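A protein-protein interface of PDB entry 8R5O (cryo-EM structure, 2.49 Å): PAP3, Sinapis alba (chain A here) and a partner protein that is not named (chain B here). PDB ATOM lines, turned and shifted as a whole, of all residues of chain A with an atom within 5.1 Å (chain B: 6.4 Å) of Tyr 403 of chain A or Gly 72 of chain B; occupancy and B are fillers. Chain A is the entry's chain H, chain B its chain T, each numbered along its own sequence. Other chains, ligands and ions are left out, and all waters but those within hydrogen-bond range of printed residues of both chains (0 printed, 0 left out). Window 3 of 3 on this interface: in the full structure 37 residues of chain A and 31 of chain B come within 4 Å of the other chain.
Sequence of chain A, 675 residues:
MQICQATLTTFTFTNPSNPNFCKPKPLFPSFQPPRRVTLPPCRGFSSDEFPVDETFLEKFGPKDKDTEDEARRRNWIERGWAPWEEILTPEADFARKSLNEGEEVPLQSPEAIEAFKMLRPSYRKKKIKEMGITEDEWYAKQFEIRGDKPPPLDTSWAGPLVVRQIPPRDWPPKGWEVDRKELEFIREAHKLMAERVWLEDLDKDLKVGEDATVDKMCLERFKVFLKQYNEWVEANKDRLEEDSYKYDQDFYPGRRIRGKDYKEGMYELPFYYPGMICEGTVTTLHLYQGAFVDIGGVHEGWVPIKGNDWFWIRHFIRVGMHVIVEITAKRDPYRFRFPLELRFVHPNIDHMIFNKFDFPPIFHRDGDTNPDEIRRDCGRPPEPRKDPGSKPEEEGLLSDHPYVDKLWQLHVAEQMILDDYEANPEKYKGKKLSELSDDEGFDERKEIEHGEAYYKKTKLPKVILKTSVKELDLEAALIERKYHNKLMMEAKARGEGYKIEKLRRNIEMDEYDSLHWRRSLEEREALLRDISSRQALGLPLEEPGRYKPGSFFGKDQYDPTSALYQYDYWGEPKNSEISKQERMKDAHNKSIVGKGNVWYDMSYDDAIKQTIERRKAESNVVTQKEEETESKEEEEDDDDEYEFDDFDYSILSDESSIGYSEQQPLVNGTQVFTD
A ring nitrogen (NE2) of His 401 of chain A sits at hydrogen-bond distance from the backbone carbonyl oxygen (O) of Lys 70 of chain B (2.9 Å).
O of Gly 72 of chain B lies within hydrogen-bond range of SG of Cys 74 of chain B, 3.6 Å away.
OG1 of Thr 71 of chain B sits at hydrogen-bond distance from SG of Cys 74 of chain B.
The backbone carbonyl oxygen (O) of Thr 71 of chain B sits at hydrogen-bond distance from the backbone NH (N) of Tyr 128 of chain B (3.0 Å).
The backbone NH (N) of Tyr 403 of chain A sits at hydrogen-bond distance from a ring nitrogen (ND1) of His 401 of chain A, at 3.0 Å.
Among the printed residues, pairs that only touch across the chains: His 401 of chain A with Thr 71 of chain B, Pro 402 of chain A with Lys 75 of chain B, Tyr 403 of chain A with Thr 71 of chain B, Tyr 403 of chain A with Gly 72 of chain B, Tyr 403 of chain A with Lys 73 of chain B, Lys 406 of chain A with Lys 73 of chain B, Tyr 512 of chain A with Lys 70 of chain B and Tyr 512 of chain A with Thr 71 of chain B.
Tyr 403 of chain A touches just these residues of chain B: Thr 71 (3.5 Å), Gly 72 (3.5 Å) and Lys 73 (3.7 Å).
Printed residues of chain A within 4 Å of Lys 70 of chain B: His 401 (2.9 Å) and Tyr 512 (3.6 Å).
Of the printed residues of chain A, Thr 71 of chain B touches His 401, Tyr 403 and Tyr 512.
Gly 72 of chain B touches one residue of chain A.
Printed residues of chain A within 4 Å of Lys 73 of chain B: Tyr 403 (3.7 Å) and Lys 406 (3.3 Å).
Phe 124 of chain B touches none of the printed residues of chain A.
Tyr 128 of chain B touches none of the printed residues of chain A.
The nearest residue of chain B that does not touch Tyr 403 of chain A is Cys 74 of chain B (4.1 Å).
The nearest residue of chain A that does not touch Gly 72 of chain B is Tyr 512 of chain A (4.9 Å).
The nearest printed residue of chain A that does not touch Lys 73 of chain B is Pro 402 of chain A (6.0 Å).
Printed residues of chain B that touch a printed residue of chain A: Lys 70, Thr 71, Gly 72, Lys 73 and Lys 75.
Of the 9 printed residues of chain A, 5 touch a printed residue of chain B.
Hydrophobic or aromatic side chains of chain A within 4 Å of the printed part of chain B: His 401, Pro 402, Tyr 403 and Tyr 512.
Among the printed residues, 9 pairs touch across the chains.
Among the printed residues, no Asp or Glu carboxylate lies within 4 Å of a Lys or Arg side-chain nitrogen of the other chain.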
ATOM      1  N   HIS A 401     -29.592 -14.372  11.301  1.00  0.00           N
ATOM      2  CA  HIS A 401     -28.472 -15.230  10.952  1.00  0.00           C
ATOM      3  C   HIS A 401     -27.163 -14.491  11.210  1.00  0.00           C
ATOM      4  O   HIS A 401     -27.020 -13.332  10.798  1.00  0.00           O
ATOM      5  CB  HIS A 401     -28.568 -15.653   9.487  1.00  0.00           C
ATOM      6  CG  HIS A 401     -27.738 -16.850   9.146  1.00  0.00           C
ATOM      7  ND1 HIS A 401     -26.362 -16.813   9.099  1.00  0.00           N
ATOM      8  CD2 HIS A 401     -28.092 -18.116   8.822  1.00  0.00           C
ATOM      9  CE1 HIS A 401     -25.903 -18.006   8.768  1.00  0.00           C
ATOM     10  NE2 HIS A 401     -26.932 -18.814   8.594  1.00  0.00           N
ATOM     11  N   PRO A 402     -26.196 -15.110  11.892  1.00  0.00           N
ATOM     12  CA  PRO A 402     -24.940 -14.401  12.193  1.00  0.00           C
ATOM     13  C   PRO A 402     -24.148 -13.997  10.960  1.00  0.00           C
ATOM     14  O   PRO A 402     -23.349 -13.056  11.038  1.00  0.00           O
ATOM     15  CB  PRO A 402     -24.165 -15.408  13.053  1.00  0.00           C
ATOM     16  CG  PRO A 402     -24.740 -16.739  12.685  1.00  0.00           C
ATOM     17  CD  PRO A 402     -26.191 -16.489  12.408  1.00  0.00           C
ATOM     18  N   TYR A 403     -24.341 -14.671   9.828  1.00  0.00           N
ATOM     19  CA  TYR A 403     -23.620 -14.342   8.607  1.00  0.00           C
ATOM     20  C   TYR A 403     -24.174 -13.110   7.903  1.00  0.00           C
ATOM     21  O   TYR A 403     -23.517 -12.586   6.996  1.00  0.00           O
ATOM     22  CB  TYR A 403     -23.640 -15.546   7.660  1.00  0.00           C
ATOM     23  CG  TYR A 403     -22.870 -15.356   6.374  1.00  0.00           C
ATOM     24  CD1 TYR A 403     -21.530 -15.001   6.389  1.00  0.00           C
ATOM     25  CD2 TYR A 403     -23.483 -15.549   5.145  1.00  0.00           C
ATOM     26  CE1 TYR A 403     -20.825 -14.831   5.217  1.00  0.00           C
ATOM     27  CE2 TYR A 403     -22.785 -15.384   3.968  1.00  0.00           C
ATOM     28  CZ  TYR A 403     -21.457 -15.024   4.009  1.00  0.00           C
ATOM     29  OH  TYR A 403     -20.755 -14.857   2.839  1.00  0.00           O
ATOM     30  N   VAL A 404     -25.353 -12.628   8.303  1.00  0.00           N
ATOM     31  CA  VAL A 404     -25.954 -11.467   7.652  1.00  0.00           C
ATOM     32  C   VAL A 404     -25.070 -10.236   7.823  1.00  0.00           C
ATOM     33  O   VAL A 404     -24.928  -9.423   6.901  1.00  0.00           O
ATOM     34  CB  VAL A 404     -27.376 -11.234   8.194  1.00  0.00           C
ATOM     35  CG1 VAL A 404     -27.837  -9.815   7.920  1.00  0.00           C
ATOM     36  CG2 VAL A 404     -28.337 -12.230   7.575  1.00  0.00           C
ATOM     37  N   ASP A 405     -24.456 -10.085   8.999  1.00  0.00           N
ATOM     38  CA  ASP A 405     -23.555  -8.958   9.223  1.00  0.00           C
ATOM     39  C   ASP A 405     -22.388  -8.967   8.245  1.00  0.00           C
ATOM     40  O   ASP A 405     -21.898  -7.902   7.856  1.00  0.00           O
ATOM     41  CB  ASP A 405     -23.041  -8.976  10.663  1.00  0.00           C
ATOM     42  CG  ASP A 405     -24.162  -8.923  11.682  1.00  0.00           C
ATOM     43  OD1 ASP A 405     -25.342  -8.920  11.274  1.00  0.00           O
ATOM     44  OD2 ASP A 405     -23.862  -8.882  12.894  1.00  0.00           O
ATOM     45  N   LYS A 406     -21.929 -10.153   7.840  1.00  0.00           N
ATOM     46  CA  LYS A 406     -20.877 -10.230   6.831  1.00  0.00           C
ATOM     47  C   LYS A 406     -21.417  -9.897   5.446  1.00  0.00           C
ATOM     48  O   LYS A 406     -20.741  -9.229   4.655  1.00  0.00           O
ATOM     49  CB  LYS A 406     -20.240 -11.618   6.842  1.00  0.00           C
ATOM     50  CG  LYS A 406     -19.085 -11.773   5.871  1.00  0.00           C
ATOM     51  CD  LYS A 406     -17.949 -10.821   6.206  1.00  0.00           C
ATOM     52  CE  LYS A 406     -16.846 -10.894   5.164  1.00  0.00           C
ATOM     53  NZ  LYS A 406     -16.330 -12.280   4.995  1.00  0.00           N
ATOM     54  N   LEU A 407     -22.630 -10.360   5.132  1.00  0.00           N
ATOM     55  CA  LEU A 407     -23.242 -10.031   3.849  1.00  0.00           C
ATOM     56  C   LEU A 407     -23.464  -8.531   3.712  1.00  0.00           C
ATOM     57  O   LEU A 407     -23.310  -7.969   2.621  1.00  0.00           O
ATOM     58  CB  LEU A 407     -24.564 -10.778   3.688  1.00  0.00           C
ATOM     59  CG  LEU A 407     -24.497 -12.276   3.402  1.00  0.00           C
ATOM     60  CD1 LEU A 407     -25.889 -12.873   3.437  1.00  0.00           C
ATOM     61  CD2 LEU A 407     -23.838 -12.530   2.057  1.00  0.00           C
ATOM     62  N   LEU A 410     -20.238  -6.866   2.639  1.00  0.00           N
ATOM     63  CA  LEU A 410     -20.000  -7.105   1.219  1.00  0.00           C
ATOM     64  C   LEU A 410     -20.950  -6.287   0.356  1.00  0.00           C
ATOM     65  O   LEU A 410     -20.561  -5.792  -0.708  1.00  0.00           O
ATOM     66  CB  LEU A 410     -20.141  -8.595   0.907  1.00  0.00           C
ATOM     67  CG  LEU A 410     -19.274  -9.554   1.723  1.00  0.00           C
ATOM     68  CD1 LEU A 410     -19.504 -10.987   1.279  1.00  0.00           C
ATOM     69  CD2 LEU A 410     -17.803  -9.186   1.619  1.00  0.00           C
ATOM     70  N   TYR A 512     -30.991 -16.200   4.139  1.00  0.00           N
ATOM     71  CA  TYR A 512     -30.206 -16.690   5.267  1.00  0.00           C
ATOM     72  C   TYR A 512     -30.979 -16.552   6.572  1.00  0.00           C
ATOM     73  O   TYR A 512     -30.890 -17.421   7.447  1.00  0.00           O
ATOM     74  CB  TYR A 512     -28.871 -15.952   5.347  1.00  0.00           C
ATOM     75  CG  TYR A 512     -27.794 -16.549   4.472  1.00  0.00           C
ATOM     76  CD1 TYR A 512     -27.055 -17.641   4.900  1.00  0.00           C
ATOM     77  CD2 TYR A 512     -27.516 -16.021   3.220  1.00  0.00           C
ATOM     78  CE1 TYR A 512     -26.070 -18.191   4.106  1.00  0.00           C
ATOM     79  CE2 TYR A 512     -26.532 -16.563   2.418  1.00  0.00           C
ATOM     80  CZ  TYR A 512     -25.812 -17.649   2.868  1.00  0.00           C
ATOM     81  OH  TYR A 512     -24.830 -18.196   2.076  1.00  0.00           O
ATOM     82  N   LYS B  70     -27.016 -23.286   6.174  1.00  0.00           N
ATOM     83  CA  LYS B  70     -25.736 -22.944   5.573  1.00  0.00           C
ATOM     84  C   LYS B  70     -25.291 -21.579   6.071  1.00  0.00           C
ATOM     85  O   LYS B  70     -26.086 -20.793   6.590  1.00  0.00           O
ATOM     86  CB  LYS B  70     -25.806 -22.957   4.040  1.00  0.00           C
ATOM     87  CG  LYS B  70     -26.689 -21.886   3.443  1.00  0.00           C
ATOM     88  CD  LYS B  70     -26.761 -22.020   1.932  1.00  0.00           C
ATOM     89  CE  LYS B  70     -27.344 -23.361   1.528  1.00  0.00           C
ATOM     90  NZ  LYS B  70     -28.698 -23.571   2.112  1.00  0.00           N
ATOM     91  N   THR B  71     -23.998 -21.309   5.913  1.00  0.00           N
ATOM     92  CA  THR B  71     -23.411 -20.066   6.392  1.00  0.00           C
ATOM     93  C   THR B  71     -22.092 -19.832   5.675  1.00  0.00           C
ATOM     94  O   THR B  71     -21.570 -20.706   4.983  1.00  0.00           O
ATOM     95  CB  THR B  71     -23.191 -20.096   7.909  1.00  0.00           C
ATOM     96  OG1 THR B  71     -22.710 -18.820   8.350  1.00  0.00           O
ATOM     97  CG2 THR B  71     -22.175 -21.162   8.275  1.00  0.00           C
ATOM     98  N   GLY B  72     -21.562 -18.626   5.853  1.00  0.00           N
ATOM     99  CA  GLY B  72     -20.216 -18.308   5.423  1.00  0.00           C
ATOM    100  C   GLY B  72     -19.305 -18.131   6.618  1.00  0.00           C
ATOM    101  O   GLY B  72     -19.550 -18.707   7.681  1.00  0.00           O
ATOM    102  N   LYS B  73     -18.252 -17.334   6.463  1.00  0.00           N
ATOM    103  CA  LYS B  73     -17.329 -17.060   7.559  1.00  0.00           C
ATOM    104  C   LYS B  73     -18.030 -16.220   8.620  1.00  0.00           C
ATOM    105  O   LYS B  73     -18.360 -15.055   8.380  1.00  0.00           O
ATOM    106  CB  LYS B  73     -16.089 -16.351   7.025  1.00  0.00           C
ATOM    107  CG  LYS B  73     -15.155 -15.821   8.097  1.00  0.00           C
ATOM    108  CD  LYS B  73     -13.850 -15.336   7.491  1.00  0.00           C
ATOM    109  CE  LYS B  73     -14.093 -14.333   6.376  1.00  0.00           C
ATOM    110  NZ  LYS B  73     -12.823 -13.896   5.734  1.00  0.00           N
ATOM    111  N   CYS B  74     -18.256 -16.805   9.793  1.00  0.00           N
ATOM    112  CA  CYS B  74     -18.951 -16.121  10.880  1.00  0.00           C
ATOM    113  C   CYS B  74     -18.730 -16.908  12.166  1.00  0.00           C
ATOM    114  O   CYS B  74     -18.000 -17.902  12.196  1.00  0.00           O
ATOM    115  CB  CYS B  74     -20.445 -15.964  10.582  1.00  0.00           C
ATOM    116  SG  CYS B  74     -21.375 -17.510  10.603  1.00  0.00           S
ATOM    117  N   LYS B  75     -19.379 -16.450  13.234  1.00  0.00           N
ATOM    118  CA  LYS B  75     -19.305 -17.074  14.548  1.00  0.00           C
ATOM    119  C   LYS B  75     -20.711 -17.165  15.122  1.00  0.00           C
ATOM    120  O   LYS B  75     -21.430 -16.164  15.159  1.00  0.00           O
ATOM    121  CB  LYS B  75     -18.393 -16.270  15.482  1.00  0.00           C
ATOM    122  CG  LYS B  75     -18.526 -16.606  16.956  1.00  0.00           C
ATOM    123  CD  LYS B  75     -17.999 -15.459  17.804  1.00  0.00           C
ATOM    124  CE  LYS B  75     -18.238 -15.691  19.283  1.00  0.00           C
ATOM    125  NZ  LYS B  75     -17.281 -16.668  19.860  1.00  0.00           N
ATOM    126  N   PHE B 124     -16.939 -20.635  11.757  1.00  0.00           N
ATOM    127  CA  PHE B 124     -16.813 -20.985  10.353  1.00  0.00           C
ATOM    128  C   PHE B 124     -15.838 -20.024   9.689  1.00  0.00           C
ATOM    129  O   PHE B 124     -15.782 -18.839  10.028  1.00  0.00           O
ATOM    130  CB  PHE B 124     -18.171 -20.939   9.642  1.00  0.00           C
ATOM    131  CG  PHE B 124     -19.258 -21.684  10.360  1.00  0.00           C
ATOM    132  CD1 PHE B 124     -20.037 -21.050  11.313  1.00  0.00           C
ATOM    133  CD2 PHE B 124     -19.502 -23.016  10.080  1.00  0.00           C
ATOM    134  CE1 PHE B 124     -21.036 -21.733  11.975  1.00  0.00           C
ATOM    135  CE2 PHE B 124     -20.502 -23.701  10.737  1.00  0.00           C
ATOM    136  CZ  PHE B 124     -21.270 -23.060  11.686  1.00  0.00           C
ATOM    137  N   ASN B 125     -15.062 -20.545   8.742  1.00  0.00           N
ATOM    138  CA  ASN B 125     -14.062 -19.753   8.046  1.00  0.00           C
ATOM    139  C   ASN B 125     -14.190 -19.842   6.533  1.00  0.00           C
ATOM    140  O   ASN B 125     -13.334 -19.304   5.822  1.00  0.00           O
ATOM    141  CB  ASN B 125     -12.650 -20.190   8.467  1.00  0.00           C
ATOM    142  CG  ASN B 125     -11.645 -19.058   8.407  1.00  0.00           C
ATOM    143  OD1 ASN B 125     -11.971 -17.907   8.692  1.00  0.00           O
ATOM    144  ND2 ASN B 125     -10.413 -19.380   8.036  1.00  0.00           N
ATOM    145  N   ALA B 126     -15.230 -20.490   6.026  1.00  0.00           N
ATOM    146  CA  ALA B 126     -15.420 -20.761   4.610  1.00  0.00           C
ATOM    147  C   ALA B 126     -16.874 -21.167   4.406  1.00  0.00           C
ATOM    148  O   ALA B 126     -17.592 -21.362   5.395  1.00  0.00           O
ATOM    149  CB  ALA B 126     -14.457 -21.856   4.144  1.00  0.00           C
ATOM    150  N   PRO B 127     -17.359 -21.283   3.167  1.00  0.00           N
ATOM    151  CA  PRO B 127     -18.740 -21.740   2.969  1.00  0.00           C
ATOM    152  C   PRO B 127     -18.989 -23.087   3.633  1.00  0.00           C
ATOM    153  O   PRO B 127     -18.170 -24.005   3.554  1.00  0.00           O
ATOM    154  CB  PRO B 127     -18.864 -21.831   1.447  1.00  0.00           C
ATOM    155  CG  PRO B 127     -17.936 -20.793   0.954  1.00  0.00           C
ATOM    156  CD  PRO B 127     -16.770 -20.791   1.908  1.00  0.00           C
ATOM    157  N   TYR B 128     -20.137 -23.191   4.292  1.00  0.00           N
ATOM    158  CA  TYR B 128     -20.498 -24.358   5.079  1.00  0.00           C
ATOM    159  C   TYR B 128     -21.948 -24.715   4.794  1.00  0.00           C
ATOM    160  O   TYR B 128     -22.792 -23.827   4.650  1.00  0.00           O
ATOM    161  CB  TYR B 128     -20.289 -24.088   6.575  1.00  0.00           C
ATOM    162  CG  TYR B 128     -20.835 -25.147   7.504  1.00  0.00           C
ATOM    163  CD1 TYR B 128     -22.134 -25.072   7.987  1.00  0.00           C
ATOM    164  CD2 TYR B 128     -20.043 -26.207   7.922  1.00  0.00           C
ATOM    165  CE1 TYR B 128     -22.633 -26.028   8.839  1.00  0.00           C
ATOM    166  CE2 TYR B 128     -20.534 -27.167   8.777  1.00  0.00           C
ATOM    167  CZ  TYR B 128     -21.830 -27.073   9.233  1.00  0.00           C
ATOM    168  OH  TYR B 128     -22.325 -28.028  10.087  1.00  0.00           O
